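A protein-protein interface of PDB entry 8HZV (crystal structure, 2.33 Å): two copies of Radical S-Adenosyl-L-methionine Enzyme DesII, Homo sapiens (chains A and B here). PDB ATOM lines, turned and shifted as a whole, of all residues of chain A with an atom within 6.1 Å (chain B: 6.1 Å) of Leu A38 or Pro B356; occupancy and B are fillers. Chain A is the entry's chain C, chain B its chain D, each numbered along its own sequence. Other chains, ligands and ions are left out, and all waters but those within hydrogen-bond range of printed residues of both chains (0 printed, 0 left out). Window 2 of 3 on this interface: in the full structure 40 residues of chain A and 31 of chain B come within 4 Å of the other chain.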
ATOM      1  N   THR A  32     -16.330   5.955 -16.334  1.00  0.00           N
ATOM      2  CA  THR A  32     -17.687   5.579 -16.715  1.00  0.00           C
ATOM      3  C   THR A  32     -18.674   6.686 -16.372  1.00  0.00           C
ATOM      4  O   THR A  32     -19.567   7.003 -17.167  1.00  0.00           O
ATOM      5  CB  THR A  32     -18.090   4.276 -16.020  1.00  0.00           C
ATOM      6  OG1 THR A  32     -17.116   3.262 -16.293  1.00  0.00           O
ATOM      7  CG2 THR A  32     -19.453   3.809 -16.507  1.00  0.00           C
ATOM      8  N   LEU A  33     -18.527   7.288 -15.190  1.00  0.00           N
ATOM      9  CA  LEU A  33     -19.417   8.375 -14.793  1.00  0.00           C
ATOM     10  C   LEU A  33     -19.251   9.590 -15.699  1.00  0.00           C
ATOM     11  O   LEU A  33     -20.242  10.213 -16.098  1.00  0.00           O
ATOM     12  CB  LEU A  33     -19.154   8.761 -13.338  1.00  0.00           C
ATOM     13  CG  LEU A  33     -19.511   7.765 -12.234  1.00  0.00           C
ATOM     14  CD1 LEU A  33     -19.224   8.376 -10.871  1.00  0.00           C
ATOM     15  CD2 LEU A  33     -20.967   7.334 -12.333  1.00  0.00           C
ATOM     16  N   ALA A  34     -18.006   9.937 -16.038  1.00  0.00           N
ATOM     17  CA  ALA A  34     -17.754  11.157 -16.796  1.00  0.00           C
ATOM     18  C   ALA A  34     -18.006  10.962 -18.286  1.00  0.00           C
ATOM     19  O   ALA A  34     -18.622  11.822 -18.927  1.00  0.00           O
ATOM     20  CB  ALA A  34     -16.322  11.639 -16.561  1.00  0.00           C
ATOM     21  N   ALA A  35     -17.532   9.850 -18.856  1.00  0.00           N
ATOM     22  CA  ALA A  35     -17.740   9.606 -20.281  1.00  0.00           C
ATOM     23  C   ALA A  35     -19.224   9.561 -20.620  1.00  0.00           C
ATOM     24  O   ALA A  35     -19.657  10.149 -21.618  1.00  0.00           O
ATOM     25  CB  ALA A  35     -17.053   8.308 -20.705  1.00  0.00           C
ATOM     26  N   GLY A  36     -20.018   8.884 -19.796  1.00  0.00           N
ATOM     27  CA  GLY A  36     -21.448   8.794 -20.006  1.00  0.00           C
ATOM     28  C   GLY A  36     -22.247  10.024 -19.638  1.00  0.00           C
ATOM     29  O   GLY A  36     -23.469  10.030 -19.811  1.00  0.00           O
ATOM     30  N   GLY A  37     -21.595  11.067 -19.130  1.00  0.00           N
ATOM     31  CA  GLY A  37     -22.302  12.282 -18.775  1.00  0.00           C
ATOM     32  C   GLY A  37     -23.248  12.150 -17.607  1.00  0.00           C
ATOM     33  O   GLY A  37     -24.195  12.934 -17.500  1.00  0.00           O
ATOM     34  N   LEU A  38     -23.023  11.176 -16.724  1.00  0.00           N
ATOM     35  CA  LEU A  38     -23.890  11.000 -15.564  1.00  0.00           C
ATOM     36  C   LEU A  38     -23.585  12.008 -14.464  1.00  0.00           C
ATOM     37  O   LEU A  38     -24.493  12.416 -13.732  1.00  0.00           O
ATOM     38  CB  LEU A  38     -23.756   9.576 -15.021  1.00  0.00           C
ATOM     39  CG  LEU A  38     -24.262   8.451 -15.927  1.00  0.00           C
ATOM     40  CD1 LEU A  38     -23.571   7.132 -15.601  1.00  0.00           C
ATOM     41  CD2 LEU A  38     -25.770   8.310 -15.823  1.00  0.00           C
ATOM     42  N   VAL A  39     -22.325  12.409 -14.330  1.00  0.00           N
ATOM     43  CA  VAL A  39     -21.878  13.319 -13.278  1.00  0.00           C
ATOM     44  C   VAL A  39     -20.946  14.342 -13.919  1.00  0.00           C
ATOM     45  O   VAL A  39     -20.205  13.995 -14.851  1.00  0.00           O
ATOM     46  CB  VAL A  39     -21.177  12.554 -12.139  1.00  0.00           C
ATOM     47  CG1 VAL A  39     -20.773  13.491 -11.012  1.00  0.00           C
ATOM     48  CG2 VAL A  39     -22.069  11.447 -11.601  1.00  0.00           C
ATOM     49  N   PRO A  40     -20.958  15.603 -13.489  1.00  0.00           N
ATOM     50  CA  PRO A  40     -19.972  16.551 -13.992  1.00  0.00           C
ATOM     51  C   PRO A  40     -18.559  16.069 -13.680  1.00  0.00           C
ATOM     52  O   PRO A  40     -18.347  15.316 -12.717  1.00  0.00           O
ATOM     53  CB  PRO A  40     -20.310  17.846 -13.246  1.00  0.00           C
ATOM     54  CG  PRO A  40     -21.782  17.739 -13.004  1.00  0.00           C
ATOM     55  CD  PRO A  40     -22.035  16.277 -12.736  1.00  0.00           C
ATOM     56  N   LEU A  86     -27.238   6.421  -9.460  1.00  0.00           N
ATOM     57  CA  LEU A  86     -25.993   6.310 -10.213  1.00  0.00           C
ATOM     58  C   LEU A  86     -25.420   4.898 -10.153  1.00  0.00           C
ATOM     59  O   LEU A  86     -24.798   4.443 -11.118  1.00  0.00           O
ATOM     60  CB  LEU A  86     -24.970   7.322  -9.692  1.00  0.00           C
ATOM     61  CG  LEU A  86     -25.208   8.785 -10.083  1.00  0.00           C
ATOM     62  CD1 LEU A  86     -24.444   9.727  -9.165  1.00  0.00           C
ATOM     63  CD2 LEU A  86     -24.836   9.022 -11.538  1.00  0.00           C
ATOM     64  N   GLN A  89     -26.381   2.638 -12.886  1.00  0.00           N
ATOM     65  CA  GLN A  89     -25.860   2.999 -14.195  1.00  0.00           C
ATOM     66  C   GLN A  89     -24.435   2.518 -14.426  1.00  0.00           C
ATOM     67  O   GLN A  89     -23.870   2.787 -15.493  1.00  0.00           O
ATOM     68  CB  GLN A  89     -25.930   4.518 -14.386  1.00  0.00           C
ATOM     69  CG  GLN A  89     -27.261   5.011 -14.932  1.00  0.00           C
ATOM     70  CD  GLN A  89     -27.791   6.208 -14.171  1.00  0.00           C
ATOM     71  OE1 GLN A  89     -27.166   6.673 -13.221  1.00  0.00           O
ATOM     72  NE2 GLN A  89     -28.943   6.719 -14.591  1.00  0.00           N
ATOM     73  N   VAL A  90     -23.835   1.832 -13.457  1.00  0.00           N
ATOM     74  CA  VAL A  90     -22.502   1.258 -13.622  1.00  0.00           C
ATOM     75  C   VAL A  90     -22.614  -0.255 -13.487  1.00  0.00           C
ATOM     76  O   VAL A  90     -22.523  -0.784 -12.370  1.00  0.00           O
ATOM     77  CB  VAL A  90     -21.505   1.836 -12.607  1.00  0.00           C
ATOM     78  CG1 VAL A  90     -20.080   1.505 -13.023  1.00  0.00           C
ATOM     79  CG2 VAL A  90     -21.697   3.341 -12.474  1.00  0.00           C
ATOM     80  N   PRO A  91     -22.803  -0.987 -14.589  1.00  0.00           N
ATOM     81  CA  PRO A  91     -23.092  -2.427 -14.474  1.00  0.00           C
ATOM     82  C   PRO A  91     -21.969  -3.225 -13.838  1.00  0.00           C
ATOM     83  O   PRO A  91     -22.230  -4.286 -13.255  1.00  0.00           O
ATOM     84  CB  PRO A  91     -23.334  -2.856 -15.929  1.00  0.00           C
ATOM     85  CG  PRO A  91     -23.611  -1.583 -16.677  1.00  0.00           C
ATOM     86  CD  PRO A  91     -22.803  -0.530 -15.989  1.00  0.00           C
ATOM     87  N   GLY B 312     -31.469  12.638 -15.278  1.00  0.00           N
ATOM     88  CA  GLY B 312     -30.772  11.559 -14.605  1.00  0.00           C
ATOM     89  C   GLY B 312     -31.540  10.266 -14.506  1.00  0.00           C
ATOM     90  O   GLY B 312     -31.093   9.344 -13.814  1.00  0.00           O
ATOM     91  N   THR B 314     -32.678   7.336 -16.867  1.00  0.00           N
ATOM     92  CA  THR B 314     -32.287   6.896 -18.198  1.00  0.00           C
ATOM     93  C   THR B 314     -33.179   5.770 -18.711  1.00  0.00           C
ATOM     94  O   THR B 314     -33.853   5.075 -17.947  1.00  0.00           O
ATOM     95  CB  THR B 314     -30.830   6.432 -18.205  1.00  0.00           C
ATOM     96  OG1 THR B 314     -30.684   5.315 -17.320  1.00  0.00           O
ATOM     97  CG2 THR B 314     -29.908   7.559 -17.755  1.00  0.00           C
ATOM     98  N   VAL B 351     -22.750   3.103 -27.104  1.00  0.00           N
ATOM     99  CA  VAL B 351     -23.565   2.966 -25.902  1.00  0.00           C
ATOM    100  C   VAL B 351     -22.728   3.269 -24.662  1.00  0.00           C
ATOM    101  O   VAL B 351     -23.139   4.037 -23.787  1.00  0.00           O
ATOM    102  CB  VAL B 351     -24.197   1.563 -25.837  1.00  0.00           C
ATOM    103  CG1 VAL B 351     -24.751   1.288 -24.450  1.00  0.00           C
ATOM    104  CG2 VAL B 351     -25.295   1.431 -26.884  1.00  0.00           C
ATOM    105  N   ARG B 352     -21.523   2.694 -24.586  1.00  0.00           N
ATOM    106  CA  ARG B 352     -20.642   2.972 -23.454  1.00  0.00           C
ATOM    107  C   ARG B 352     -20.226   4.436 -23.412  1.00  0.00           C
ATOM    108  O   ARG B 352     -19.987   4.984 -22.329  1.00  0.00           O
ATOM    109  CB  ARG B 352     -19.404   2.076 -23.514  1.00  0.00           C
ATOM    110  CG  ARG B 352     -19.712   0.590 -23.574  1.00  0.00           C
ATOM    111  CD  ARG B 352     -18.463  -0.246 -23.329  1.00  0.00           C
ATOM    112  NE  ARG B 352     -17.467  -0.070 -24.384  1.00  0.00           N
ATOM    113  CZ  ARG B 352     -17.395  -0.821 -25.480  1.00  0.00           C
ATOM    114  NH1 ARG B 352     -18.266  -1.803 -25.674  1.00  0.00           N
ATOM    115  NH2 ARG B 352     -16.454  -0.587 -26.384  1.00  0.00           N
ATOM    116  N   GLU B 353     -20.136   5.085 -24.573  1.00  0.00           N
ATOM    117  CA  GLU B 353     -19.760   6.494 -24.620  1.00  0.00           C
ATOM    118  C   GLU B 353     -20.913   7.397 -24.211  1.00  0.00           C
ATOM    119  O   GLU B 353     -20.705   8.431 -23.566  1.00  0.00           O
ATOM    120  CB  GLU B 353     -19.309   6.866 -26.034  1.00  0.00           C
ATOM    121  CG  GLU B 353     -17.812   6.720 -26.294  1.00  0.00           C
ATOM    122  CD  GLU B 353     -17.478   6.710 -27.779  1.00  0.00           C
ATOM    123  OE1 GLU B 353     -16.545   5.980 -28.176  1.00  0.00           O
ATOM    124  OE2 GLU B 353     -18.151   7.431 -28.548  1.00  0.00           O
ATOM    125  N   ARG B 354     -22.132   7.031 -24.588  1.00  0.00           N
ATOM    126  CA  ARG B 354     -23.278   7.923 -24.489  1.00  0.00           C
ATOM    127  C   ARG B 354     -24.377   7.473 -23.542  1.00  0.00           C
ATOM    128  O   ARG B 354     -25.014   8.323 -22.921  1.00  0.00           O
ATOM    129  CB  ARG B 354     -23.916   8.108 -25.883  1.00  0.00           C
ATOM    130  CG  ARG B 354     -23.282   9.227 -26.725  1.00  0.00           C
ATOM    131  CD  ARG B 354     -22.537   8.635 -27.892  1.00  0.00           C
ATOM    132  NE  ARG B 354     -21.900   9.662 -28.692  1.00  0.00           N
ATOM    133  CZ  ARG B 354     -22.581  10.588 -29.344  1.00  0.00           C
ATOM    134  NH1 ARG B 354     -21.943  11.490 -30.068  1.00  0.00           N
ATOM    135  NH2 ARG B 354     -23.904  10.620 -29.241  1.00  0.00           N
ATOM    136  N   THR B 355     -24.611   6.167 -23.421  1.00  0.00           N
ATOM    137  CA  THR B 355     -25.703   5.634 -22.604  1.00  0.00           C
ATOM    138  C   THR B 355     -25.205   4.413 -21.837  1.00  0.00           C
ATOM    139  O   THR B 355     -25.672   3.289 -22.049  1.00  0.00           O
ATOM    140  CB  THR B 355     -26.903   5.273 -23.482  1.00  0.00           C
ATOM    141  OG1 THR B 355     -26.496   4.295 -24.444  1.00  0.00           O
ATOM    142  CG2 THR B 355     -27.445   6.508 -24.216  1.00  0.00           C
ATOM    143  N   PRO B 356     -24.257   4.603 -20.912  1.00  0.00           N
ATOM    144  CA  PRO B 356     -23.510   3.450 -20.377  1.00  0.00           C
ATOM    145  C   PRO B 356     -24.349   2.483 -19.557  1.00  0.00           C
ATOM    146  O   PRO B 356     -23.892   1.360 -19.307  1.00  0.00           O
ATOM    147  CB  PRO B 356     -22.421   4.105 -19.519  1.00  0.00           C
ATOM    148  CG  PRO B 356     -23.003   5.424 -19.120  1.00  0.00           C
ATOM    149  CD  PRO B 356     -23.844   5.872 -20.285  1.00  0.00           C
ATOM    150  N   GLY B 357     -25.550   2.866 -19.141  1.00  0.00           N
ATOM    151  CA  GLY B 357     -26.416   1.988 -18.391  1.00  0.00           C
ATOM    152  C   GLY B 357     -27.430   1.220 -19.208  1.00  0.00           C
ATOM    153  O   GLY B 357     -28.199   0.442 -18.639  1.00  0.00           O
ATOM    154  N   LEU B 358     -27.453   1.405 -20.526  1.00  0.00           N
ATOM    155  CA  LEU B 358     -28.471   0.787 -21.366  1.00  0.00           C
ATOM    156  C   LEU B 358     -28.201  -0.705 -21.524  1.00  0.00           C
ATOM    157  O   LEU B 358     -27.132  -1.104 -21.997  1.00  0.00           O
ATOM    158  CB  LEU B 358     -28.504   1.475 -22.729  1.00  0.00           C
ATOM    159  CG  LEU B 358     -29.614   1.083 -23.703  1.00  0.00           C
ATOM    160  CD1 LEU B 358     -30.971   1.534 -23.188  1.00  0.00           C
ATOM    161  CD2 LEU B 358     -29.337   1.679 -25.075  1.00  0.00           C
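NE2 of Gln A89 lies within hydrogen-bond range of O of Gly B312 (3.5 Å).
O of Ala A35 lies close to O of Glu B353 (2.8 Å).
The backbone NH (N) of Leu A38 lies within hydrogen-bond range of the backbone carbonyl oxygen (O) of Leu A33.
Gly A36 touches Glu B353 (CA to O, 3.7 Å).
Gly A36 touches Arg B354 (O to O, 3.9 Å).
CD of Pro B356 touches CA of Gly A36, 3.8 Å away.
Leu A38 touches Pro B356 (CD1 to CG, 3.95 Å).
CG2 of Thr B314 touches NE2 of Gln A89, 3.4 Å away.
Gln A89 touches Gly B357 (O to CA, 3.9 Å).
CG of Pro A91 touches O of Pro B356 (3.96 Å).
Of chain B, only Pro B356 comes within 4 Å of Leu A38.
Pro B356 touches just these residues of chain A: Gly A36, Leu A38 and Pro A91.
Of the printed residues of chain A, Glu B353 touches Ala A35 and Gly A36.
Of the printed residues of chain A, Gly B312 touches Gln A89 (3.5 Å).
Printed residues of chain A within 4 Å of Arg B354: Gly A36 (3.9 Å).
Gly A37 touches none of the printed residues of chain B.
The nearest residue of chain A that does not touch Pro B356 is Gln A89 (4.1 Å).
Hydrophobic or aromatic side chains of chain B that line the printed part of chain A: Pro B356.
Among the printed residues, no Asp or Glu carboxylate lies within 4 Å of a Lys or Arg side-chain nitrogen of the other chain.
No position is printed for both chains.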
